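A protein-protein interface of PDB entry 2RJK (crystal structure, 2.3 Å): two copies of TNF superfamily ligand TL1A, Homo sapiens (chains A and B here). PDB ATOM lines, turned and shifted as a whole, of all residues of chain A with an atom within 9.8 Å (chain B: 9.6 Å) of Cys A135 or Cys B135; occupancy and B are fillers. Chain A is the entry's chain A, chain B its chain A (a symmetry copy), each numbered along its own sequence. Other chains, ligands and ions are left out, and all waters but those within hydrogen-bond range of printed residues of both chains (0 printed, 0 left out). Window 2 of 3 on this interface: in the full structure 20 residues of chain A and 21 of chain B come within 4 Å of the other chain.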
ATOM      1  N   LYS A 106     -30.944 -10.732  29.982  1.00  0.00           N
ATOM      2  CA  LYS A 106     -32.378 -10.871  30.264  1.00  0.00           C
ATOM      3  C   LYS A 106     -33.132  -9.522  30.188  1.00  0.00           C
ATOM      4  O   LYS A 106     -33.967  -9.342  29.292  1.00  0.00           O
ATOM      5  CB  LYS A 106     -32.617 -11.603  31.600  1.00  0.00           C
ATOM      6  CG  LYS A 106     -34.083 -11.900  31.929  1.00  0.00           C
ATOM      7  CD  LYS A 106     -34.279 -12.228  33.416  1.00  0.00           C
ATOM      8  CE  LYS A 106     -34.246 -13.731  33.688  1.00  0.00           C
ATOM      9  NZ  LYS A 106     -32.939 -14.351  33.343  1.00  0.00           N
ATOM     10  N   PRO A 107     -32.812  -8.554  31.085  1.00  0.00           N
ATOM     11  CA  PRO A 107     -33.535  -7.276  31.055  1.00  0.00           C
ATOM     12  C   PRO A 107     -33.107  -6.470  29.822  1.00  0.00           C
ATOM     13  O   PRO A 107     -31.959  -6.554  29.403  1.00  0.00           O
ATOM     14  CB  PRO A 107     -33.036  -6.580  32.320  1.00  0.00           C
ATOM     15  CG  PRO A 107     -31.616  -7.047  32.421  1.00  0.00           C
ATOM     16  CD  PRO A 107     -31.735  -8.528  32.096  1.00  0.00           C
ATOM     17  N   ASP A 108     -34.014  -5.706  29.233  1.00  0.00           N
ATOM     18  CA  ASP A 108     -33.615  -4.881  28.108  1.00  0.00           C
ATOM     19  C   ASP A 108     -32.801  -3.659  28.551  1.00  0.00           C
ATOM     20  O   ASP A 108     -31.875  -3.237  27.850  1.00  0.00           O
ATOM     21  CB  ASP A 108     -34.834  -4.456  27.298  1.00  0.00           C
ATOM     22  CG  ASP A 108     -35.119  -5.406  26.149  1.00  0.00           C
ATOM     23  OD1 ASP A 108     -34.142  -5.894  25.515  1.00  0.00           O
ATOM     24  OD2 ASP A 108     -36.320  -5.660  25.881  1.00  0.00           O
ATOM     25  N   SER A 109     -33.136  -3.122  29.732  1.00  0.00           N
ATOM     26  CA  SER A 109     -32.483  -1.944  30.278  1.00  0.00           C
ATOM     27  C   SER A 109     -32.527  -1.976  31.792  1.00  0.00           C
ATOM     28  O   SER A 109     -33.235  -2.796  32.401  1.00  0.00           O
ATOM     29  CB  SER A 109     -33.247  -0.714  29.815  1.00  0.00           C
ATOM     30  OG  SER A 109     -34.537  -0.740  30.415  1.00  0.00           O
ATOM     31  N   ILE A 110     -31.781  -1.058  32.395  1.00  0.00           N
ATOM     32  CA  ILE A 110     -31.759  -0.876  33.846  1.00  0.00           C
ATOM     33  C   ILE A 110     -32.024   0.600  34.081  1.00  0.00           C
ATOM     34  O   ILE A 110     -31.616   1.436  33.271  1.00  0.00           O
ATOM     35  CB  ILE A 110     -30.388  -1.270  34.440  1.00  0.00           C
ATOM     36  CG1 ILE A 110     -29.295  -0.619  33.585  1.00  0.00           C
ATOM     37  CG2 ILE A 110     -30.236  -2.836  34.479  1.00  0.00           C
ATOM     38  CD1 ILE A 110     -27.838  -0.865  34.000  1.00  0.00           C
ATOM     39  N   LYS A 132     -30.379   2.990  31.234  1.00  0.00           N
ATOM     40  CA  LYS A 132     -29.338   2.571  30.341  1.00  0.00           C
ATOM     41  C   LYS A 132     -29.789   1.251  29.738  1.00  0.00           C
ATOM     42  O   LYS A 132     -30.171   0.336  30.462  1.00  0.00           O
ATOM     43  CB  LYS A 132     -28.037   2.390  31.123  1.00  0.00           C
ATOM     44  CG  LYS A 132     -26.921   1.957  30.267  1.00  0.00           C
ATOM     45  CD  LYS A 132     -25.593   2.281  30.885  1.00  0.00           C
ATOM     46  CE  LYS A 132     -24.487   2.028  29.840  1.00  0.00           C
ATOM     47  NZ  LYS A 132     -24.847   0.861  28.959  1.00  0.00           N
ATOM     48  N   SER A 133     -29.795   1.147  28.415  1.00  0.00           N
ATOM     49  CA  SER A 133     -30.173  -0.128  27.825  1.00  0.00           C
ATOM     50  C   SER A 133     -29.005  -1.105  28.002  1.00  0.00           C
ATOM     51  O   SER A 133     -27.857  -0.696  28.018  1.00  0.00           O
ATOM     52  CB  SER A 133     -30.674   0.030  26.385  1.00  0.00           C
ATOM     53  OG  SER A 133     -29.623   0.317  25.520  1.00  0.00           O
ATOM     54  N   VAL A 134     -29.289  -2.377  28.266  1.00  0.00           N
ATOM     55  CA  VAL A 134     -28.182  -3.296  28.604  1.00  0.00           C
ATOM     56  C   VAL A 134     -27.834  -4.249  27.455  1.00  0.00           C
ATOM     57  O   VAL A 134     -28.717  -4.792  26.762  1.00  0.00           O
ATOM     58  CB  VAL A 134     -28.349  -4.031  29.987  1.00  0.00           C
ATOM     59  CG1 VAL A 134     -29.778  -4.177  30.362  1.00  0.00           C
ATOM     60  CG2 VAL A 134     -27.686  -5.397  29.952  1.00  0.00           C
ATOM     61  N   CYS A 135     -26.531  -4.442  27.277  1.00  0.00           N
ATOM     62  CA  CYS A 135     -25.978  -4.812  25.978  1.00  0.00           C
ATOM     63  C   CYS A 135     -25.878  -6.300  25.656  1.00  0.00           C
ATOM     64  O   CYS A 135     -26.428  -6.759  24.648  1.00  0.00           O
ATOM     65  CB  CYS A 135     -24.609  -4.165  25.815  1.00  0.00           C
ATOM     66  SG  CYS A 135     -24.519  -3.112  24.380  1.00  0.00           S
ATOM     67  N   GLU A 136     -25.165  -7.047  26.491  1.00  0.00           N
ATOM     68  CA  GLU A 136     -24.879  -8.433  26.148  1.00  0.00           C
ATOM     69  C   GLU A 136     -25.834  -9.465  26.746  1.00  0.00           C
ATOM     70  O   GLU A 136     -26.532  -9.202  27.736  1.00  0.00           O
ATOM     71  CB  GLU A 136     -23.411  -8.800  26.436  1.00  0.00           C
ATOM     72  CG  GLU A 136     -23.009  -8.741  27.897  1.00  0.00           C
ATOM     73  CD  GLU A 136     -22.675  -7.332  28.357  1.00  0.00           C
ATOM     74  OE1 GLU A 136     -21.560  -7.130  28.890  1.00  0.00           O
ATOM     75  OE2 GLU A 136     -23.521  -6.427  28.179  1.00  0.00           O
ATOM     76  N   VAL A 137     -25.868 -10.628  26.090  1.00  0.00           N
ATOM     77  CA  VAL A 137     -26.600 -11.812  26.545  1.00  0.00           C
ATOM     78  C   VAL A 137     -25.731 -12.589  27.546  1.00  0.00           C
ATOM     79  O   VAL A 137     -24.502 -12.446  27.555  1.00  0.00           O
ATOM     80  CB  VAL A 137     -27.045 -12.712  25.330  1.00  0.00           C
ATOM     81  CG1 VAL A 137     -25.892 -12.934  24.344  1.00  0.00           C
ATOM     82  CG2 VAL A 137     -27.637 -14.050  25.799  1.00  0.00           C
ATOM     83  N   GLY A 138     -26.374 -13.387  28.399  1.00  0.00           N
ATOM     84  CA  GLY A 138     -25.677 -14.138  29.449  1.00  0.00           C
ATOM     85  C   GLY A 138     -26.299 -13.903  30.818  1.00  0.00           C
ATOM     86  O   GLY A 138     -27.431 -14.336  31.069  1.00  0.00           O
ATOM     87  N   SER A 139     -25.567 -13.234  31.714  1.00  0.00           N
ATOM     88  CA  SER A 139     -24.172 -12.819  31.490  1.00  0.00           C
ATOM     89  C   SER A 139     -23.557 -12.309  32.799  1.00  0.00           C
ATOM     90  O   SER A 139     -24.268 -12.079  33.788  1.00  0.00           O
ATOM     91  CB  SER A 139     -24.083 -11.734  30.412  1.00  0.00           C
ATOM     92  OG  SER A 139     -22.840 -11.786  29.729  1.00  0.00           O
ATOM     93  N   TRP A 141     -22.185  -9.303  33.278  1.00  0.00           N
ATOM     94  CA  TRP A 141     -21.990  -7.876  33.067  1.00  0.00           C
ATOM     95  C   TRP A 141     -22.195  -7.108  34.383  1.00  0.00           C
ATOM     96  O   TRP A 141     -22.875  -7.569  35.289  1.00  0.00           O
ATOM     97  CB  TRP A 141     -22.958  -7.353  32.002  1.00  0.00           C
ATOM     98  CG  TRP A 141     -24.370  -7.585  32.378  1.00  0.00           C
ATOM     99  CD1 TRP A 141     -25.111  -8.720  32.136  1.00  0.00           C
ATOM    100  CD2 TRP A 141     -25.235  -6.691  33.099  1.00  0.00           C
ATOM    101  NE1 TRP A 141     -26.386  -8.579  32.655  1.00  0.00           N
ATOM    102  CE2 TRP A 141     -26.488  -7.346  33.249  1.00  0.00           C
ATOM    103  CE3 TRP A 141     -25.082  -5.404  33.623  1.00  0.00           C
ATOM    104  CZ2 TRP A 141     -27.552  -6.763  33.913  1.00  0.00           C
ATOM    105  CZ3 TRP A 141     -26.153  -4.816  34.267  1.00  0.00           C
ATOM    106  CH2 TRP A 141     -27.359  -5.506  34.441  1.00  0.00           C
ATOM    107  N   PHE A 142     -21.599  -5.934  34.502  1.00  0.00           N
ATOM    108  CA  PHE A 142     -22.019  -5.068  35.587  1.00  0.00           C
ATOM    109  C   PHE A 142     -21.921  -3.656  35.143  1.00  0.00           C
ATOM    110  O   PHE A 142     -21.175  -3.313  34.222  1.00  0.00           O
ATOM    111  CB  PHE A 142     -21.256  -5.308  36.906  1.00  0.00           C
ATOM    112  CG  PHE A 142     -19.850  -5.668  36.705  1.00  0.00           C
ATOM    113  CD1 PHE A 142     -19.498  -6.988  36.418  1.00  0.00           C
ATOM    114  CD2 PHE A 142     -18.872  -4.696  36.728  1.00  0.00           C
ATOM    115  CE1 PHE A 142     -18.185  -7.346  36.173  1.00  0.00           C
ATOM    116  CE2 PHE A 142     -17.543  -5.030  36.502  1.00  0.00           C
ATOM    117  CZ  PHE A 142     -17.194  -6.371  36.221  1.00  0.00           C
ATOM    118  N   GLN A 143     -22.737  -2.830  35.764  1.00  0.00           N
ATOM    119  CA  GLN A 143     -22.612  -1.460  35.443  1.00  0.00           C
ATOM    120  C   GLN A 143     -23.314  -0.454  36.312  1.00  0.00           C
ATOM    121  O   GLN A 143     -24.404  -0.718  36.818  1.00  0.00           O
ATOM    122  CB  GLN A 143     -22.971  -1.292  34.041  1.00  0.00           C
ATOM    123  CG  GLN A 143     -24.366  -1.212  33.766  1.00  0.00           C
ATOM    124  CD  GLN A 143     -24.444  -1.005  32.283  1.00  0.00           C
ATOM    125  OE1 GLN A 143     -23.679  -0.192  31.748  1.00  0.00           O
ATOM    126  NE2 GLN A 143     -25.284  -1.783  31.591  1.00  0.00           N
ATOM    127  N   LYS B 106     -25.973   3.558  14.247  1.00  0.00           N
ATOM    128  CA  LYS B 106     -25.515   4.536  13.253  1.00  0.00           C
ATOM    129  C   LYS B 106     -24.271   5.326  13.725  1.00  0.00           C
ATOM    130  O   LYS B 106     -23.191   5.167  13.140  1.00  0.00           O
ATOM    131  CB  LYS B 106     -26.665   5.462  12.809  1.00  0.00           C
ATOM    132  CG  LYS B 106     -26.317   6.445  11.687  1.00  0.00           C
ATOM    133  CD  LYS B 106     -27.336   7.590  11.594  1.00  0.00           C
ATOM    134  CE  LYS B 106     -28.434   7.306  10.570  1.00  0.00           C
ATOM    135  NZ  LYS B 106     -29.251   6.113  10.916  1.00  0.00           N
ATOM    136  N   PRO B 107     -24.395   6.136  14.808  1.00  0.00           N
ATOM    137  CA  PRO B 107     -23.239   6.922  15.256  1.00  0.00           C
ATOM    138  C   PRO B 107     -22.202   5.992  15.898  1.00  0.00           C
ATOM    139  O   PRO B 107     -22.567   4.999  16.517  1.00  0.00           O
ATOM    140  CB  PRO B 107     -23.845   7.828  16.327  1.00  0.00           C
ATOM    141  CG  PRO B 107     -24.901   6.960  16.941  1.00  0.00           C
ATOM    142  CD  PRO B 107     -25.541   6.313  15.723  1.00  0.00           C
ATOM    143  N   ASP B 108     -20.921   6.292  15.748  1.00  0.00           N
ATOM    144  CA  ASP B 108     -19.923   5.466  16.404  1.00  0.00           C
ATOM    145  C   ASP B 108     -19.860   5.731  17.914  1.00  0.00           C
ATOM    146  O   ASP B 108     -19.634   4.807  18.703  1.00  0.00           O
ATOM    147  CB  ASP B 108     -18.557   5.665  15.761  1.00  0.00           C
ATOM    148  CG  ASP B 108     -18.283   4.648  14.668  1.00  0.00           C
ATOM    149  OD1 ASP B 108     -18.677   3.461  14.840  1.00  0.00           O
ATOM    150  OD2 ASP B 108     -17.673   5.039  13.642  1.00  0.00           O
ATOM    151  N   SER B 109     -20.095   6.992  18.303  1.00  0.00           N
ATOM    152  CA  SER B 109     -20.042   7.412  19.693  1.00  0.00           C
ATOM    153  C   SER B 109     -20.974   8.585  19.921  1.00  0.00           C
ATOM    154  O   SER B 109     -21.495   9.192  18.969  1.00  0.00           O
ATOM    155  CB  SER B 109     -18.627   7.875  20.000  1.00  0.00           C
ATOM    156  OG  SER B 109     -18.369   9.051  19.242  1.00  0.00           O
ATOM    157  N   ILE B 110     -21.160   8.916  21.193  1.00  0.00           N
ATOM    158  CA  ILE B 110     -21.956  10.070  21.609  1.00  0.00           C
ATOM    159  C   ILE B 110     -21.071  10.863  22.553  1.00  0.00           C
ATOM    160  O   ILE B 110     -20.267  10.277  23.282  1.00  0.00           O
ATOM    161  CB  ILE B 110     -23.247   9.630  22.335  1.00  0.00           C
ATOM    162  CG1 ILE B 110     -22.869   8.567  23.372  1.00  0.00           C
ATOM    163  CG2 ILE B 110     -24.299   9.082  21.300  1.00  0.00           C
ATOM    164  CD1 ILE B 110     -24.002   7.987  24.229  1.00  0.00           C
ATOM    165  N   LYS B 132     -18.682   8.513  24.853  1.00  0.00           N
ATOM    166  CA  LYS B 132     -18.905   7.112  25.069  1.00  0.00           C
ATOM    167  C   LYS B 132     -19.111   6.489  23.698  1.00  0.00           C
ATOM    168  O   LYS B 132     -19.924   6.971  22.912  1.00  0.00           O
ATOM    169  CB  LYS B 132     -20.148   6.921  25.939  1.00  0.00           C
ATOM    170  CG  LYS B 132     -20.441   5.503  26.201  1.00  0.00           C
ATOM    171  CD  LYS B 132     -21.288   5.332  27.427  1.00  0.00           C
ATOM    172  CE  LYS B 132     -21.348   3.831  27.778  1.00  0.00           C
ATOM    173  NZ  LYS B 132     -21.335   2.993  26.527  1.00  0.00           N
ATOM    174  N   SER B 133     -18.355   5.448  23.374  1.00  0.00           N
ATOM    175  CA  SER B 133     -18.578   4.809  22.086  1.00  0.00           C
ATOM    176  C   SER B 133     -19.864   3.980  22.177  1.00  0.00           C
ATOM    177  O   SER B 133     -20.199   3.476  23.234  1.00  0.00           O
ATOM    178  CB  SER B 133     -17.342   4.039  21.605  1.00  0.00           C
ATOM    179  OG  SER B 133     -17.159   2.876  22.346  1.00  0.00           O
ATOM    180  N   VAL B 134     -20.658   3.942  21.111  1.00  0.00           N
ATOM    181  CA  VAL B 134     -21.979   3.289  21.232  1.00  0.00           C
ATOM    182  C   VAL B 134     -22.023   1.915  20.555  1.00  0.00           C
ATOM    183  O   VAL B 134     -21.485   1.711  19.450  1.00  0.00           O
ATOM    184  CB  VAL B 134     -23.196   4.210  20.843  1.00  0.00           C
ATOM    185  CG1 VAL B 134     -22.803   5.254  19.864  1.00  0.00           C
ATOM    186  CG2 VAL B 134     -24.336   3.381  20.278  1.00  0.00           C
ATOM    187  N   CYS B 135     -22.681   0.985  21.241  1.00  0.00           N
ATOM    188  CA  CYS B 135     -22.381  -0.436  21.095  1.00  0.00           C
ATOM    189  C   CYS B 135     -23.137  -1.206  20.017  1.00  0.00           C
ATOM    190  O   CYS B 135     -22.520  -1.812  19.134  1.00  0.00           O
ATOM    191  CB  CYS B 135     -22.571  -1.126  22.439  1.00  0.00           C
ATOM    192  SG  CYS B 135     -21.090  -1.943  23.000  1.00  0.00           S
ATOM    193  N   GLU B 136     -24.463  -1.203  20.097  1.00  0.00           N
ATOM    194  CA  GLU B 136     -25.237  -2.062  19.211  1.00  0.00           C
ATOM    195  C   GLU B 136     -25.757  -1.392  17.940  1.00  0.00           C
ATOM    196  O   GLU B 136     -25.859  -0.160  17.855  1.00  0.00           O
ATOM    197  CB  GLU B 136     -26.371  -2.782  19.965  1.00  0.00           C
ATOM    198  CG  GLU B 136     -27.437  -1.872  20.543  1.00  0.00           C
ATOM    199  CD  GLU B 136     -27.031  -1.266  21.876  1.00  0.00           C
ATOM    200  OE1 GLU B 136     -27.794  -1.421  22.856  1.00  0.00           O
ATOM    201  OE2 GLU B 136     -25.948  -0.641  21.945  1.00  0.00           O
ATOM    202  N   VAL B 137     -26.042  -2.240  16.949  1.00  0.00           N
ATOM    203  CA  VAL B 137     -26.677  -1.853  15.688  1.00  0.00           C
ATOM    204  C   VAL B 137     -28.202  -1.820  15.879  1.00  0.00           C
ATOM    205  O   VAL B 137     -28.734  -2.459  16.796  1.00  0.00           O
ATOM    206  CB  VAL B 137     -26.253  -2.815  14.513  1.00  0.00           C
ATOM    207  CG1 VAL B 137     -26.355  -4.287  14.930  1.00  0.00           C
ATOM    208  CG2 VAL B 137     -27.060  -2.544  13.235  1.00  0.00           C
ATOM    209  N   GLY B 138     -28.893  -1.057  15.031  1.00  0.00           N
ATOM    210  CA  GLY B 138     -30.345  -0.882  15.137  1.00  0.00           C
ATOM    211  C   GLY B 138     -30.736   0.588  15.152  1.00  0.00           C
ATOM    212  O   GLY B 138     -30.589   1.280  14.137  1.00  0.00           O
ATOM    213  N   SER B 139     -31.248   1.073  16.288  1.00  0.00           N
ATOM    214  CA  SER B 139     -31.554   0.247  17.468  1.00  0.00           C
ATOM    215  C   SER B 139     -32.358   1.064  18.488  1.00  0.00           C
ATOM    216  O   SER B 139     -32.474   2.292  18.370  1.00  0.00           O
ATOM    217  CB  SER B 139     -30.273  -0.286  18.119  1.00  0.00           C
ATOM    218  OG  SER B 139     -30.504  -1.524  18.774  1.00  0.00           O
ATOM    219  N   TRP B 141     -31.512   1.603  21.672  1.00  0.00           N
ATOM    220  CA  TRP B 141     -30.610   1.781  22.802  1.00  0.00           C
ATOM    221  C   TRP B 141     -30.853   3.145  23.470  1.00  0.00           C
ATOM    222  O   TRP B 141     -31.353   4.075  22.853  1.00  0.00           O
ATOM    223  CB  TRP B 141     -29.151   1.675  22.348  1.00  0.00           C
ATOM    224  CG  TRP B 141     -28.820   2.684  21.317  1.00  0.00           C
ATOM    225  CD1 TRP B 141     -28.991   2.559  19.957  1.00  0.00           C
ATOM    226  CD2 TRP B 141     -28.289   4.003  21.532  1.00  0.00           C
ATOM    227  NE1 TRP B 141     -28.588   3.717  19.315  1.00  0.00           N
ATOM    228  CE2 TRP B 141     -28.154   4.616  20.257  1.00  0.00           C
ATOM    229  CE3 TRP B 141     -27.906   4.722  22.667  1.00  0.00           C
ATOM    230  CZ2 TRP B 141     -27.679   5.906  20.103  1.00  0.00           C
ATOM    231  CZ3 TRP B 141     -27.411   6.001  22.510  1.00  0.00           C
ATOM    232  CH2 TRP B 141     -27.336   6.596  21.244  1.00  0.00           C
ATOM    233  N   PHE B 142     -30.510   3.269  24.741  1.00  0.00           N
ATOM    234  CA  PHE B 142     -30.443   4.608  25.295  1.00  0.00           C
ATOM    235  C   PHE B 142     -29.359   4.657  26.307  1.00  0.00           C
ATOM    236  O   PHE B 142     -28.955   3.641  26.878  1.00  0.00           O
ATOM    237  CB  PHE B 142     -31.784   5.112  25.867  1.00  0.00           C
ATOM    238  CG  PHE B 142     -32.581   4.054  26.495  1.00  0.00           C
ATOM    239  CD1 PHE B 142     -33.382   3.222  25.711  1.00  0.00           C
ATOM    240  CD2 PHE B 142     -32.493   3.828  27.852  1.00  0.00           C
ATOM    241  CE1 PHE B 142     -34.105   2.184  26.270  1.00  0.00           C
ATOM    242  CE2 PHE B 142     -33.219   2.802  28.443  1.00  0.00           C
ATOM    243  CZ  PHE B 142     -34.036   1.970  27.644  1.00  0.00           C
ATOM    244  N   GLN B 143     -28.833   5.851  26.486  1.00  0.00           N
ATOM    245  CA  GLN B 143     -27.864   5.966  27.508  1.00  0.00           C
ATOM    246  C   GLN B 143     -27.438   7.341  27.939  1.00  0.00           C
ATOM    247  O   GLN B 143     -27.366   8.258  27.122  1.00  0.00           O
ATOM    248  CB  GLN B 143     -26.717   5.147  27.134  1.00  0.00           C
ATOM    249  CG  GLN B 143     -25.802   5.747  26.222  1.00  0.00           C
ATOM    250  CD  GLN B 143     -24.722   4.722  26.047  1.00  0.00           C
ATOM    251  OE1 GLN B 143     -24.280   4.138  27.045  1.00  0.00           O
ATOM    252  NE2 GLN B 143     -24.349   4.420  24.799  1.00  0.00           N
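The backbone carbonyl oxygen (O) of Phe B142 lies within hydrogen-bond range of the backbone NH (N) of Ser A133 (3.0 Å).
OE2 of Glu B136 lies within hydrogen-bond range of SG of Cys A135, at 3.8 Å.
The backbone NH (N) of Lys A132 lies within hydrogen-bond range of the backbone carbonyl oxygen (O) of Ile A110 (2.8 Å).
The side-chain amino group (NZ) of Lys A132 sits close to the side-chain amide oxygen (OE1) of Gln A143 (3.2 Å).
OE1 of Gln B143 sits close to NZ of Lys B132 (3.2 Å).
Among the printed residues, merely in contact across the chains: Ser A109 with Phe B142 (3.5 Å), Lys A132 with Phe B142 (3.6 Å), Lys A132 with Gln B143 (3.5 Å), Ser A133 with Glu B136 (3.7 Å), Ser A133 with Trp B141 (3.2 Å) and Cys A135 with Cys B135 (3.4 Å).
Of the printed residues of chain B, Cys A135 touches Cys B135 (3.4 Å) and Glu B136 (3.8 Å).
Of chain A, only Cys A135 comes within 4 Å of Cys B135.
No residue of chain B comes within 4 Å of Glu A136.
No residue of chain A comes within 4 Å of Val B134.
Printed residues of chain A within 4 Å of Trp B141: Ser A133 (3.2 Å).
Of the printed residues of chain B, Lys A132 touches Phe B142 and Gln B143.
Lys B106 touches none of the printed residues of chain A.
The nearest residue of chain A that does not touch Cys B135 is Lys A132 (7.2 Å).
The nearest printed residue of chain A that does not touch Gln B143 is Ser A133 (5.2 Å).
Printed residues of chain B that touch a printed residue of chain A: Cys B135, Glu B136, Trp B141, Phe B142 and Gln B143.
Of the 16 printed residues of chain A, 4 touch a printed residue of chain B.
Among the printed residues, 8 pairs touch across the chains.
Among the printed residues, no Asp or Glu carboxylate lies within 4 Å of a Lys or Arg side-chain nitrogen of the other chain.
Lys A132 touches Gln B143, but with the chains exchanged Gln A143 does not touch Lys B132 (6.1 Å).
Ser A133 touches Glu B136, but with the chains exchanged Glu A136 does not touch Ser B133 (11.6 Å).
Ser A133 touches Trp B141, but with the chains exchanged Trp A141 does not touch Ser B133 (14.2 Å).
Cys A135 touches Glu B136, but with the chains exchanged Glu A136 does not touch Cys B135 (7.3 Å).
Of the 8 pairs that touch across the chains among the printed residues, 1 has its exchanged pair printed and touching as well.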
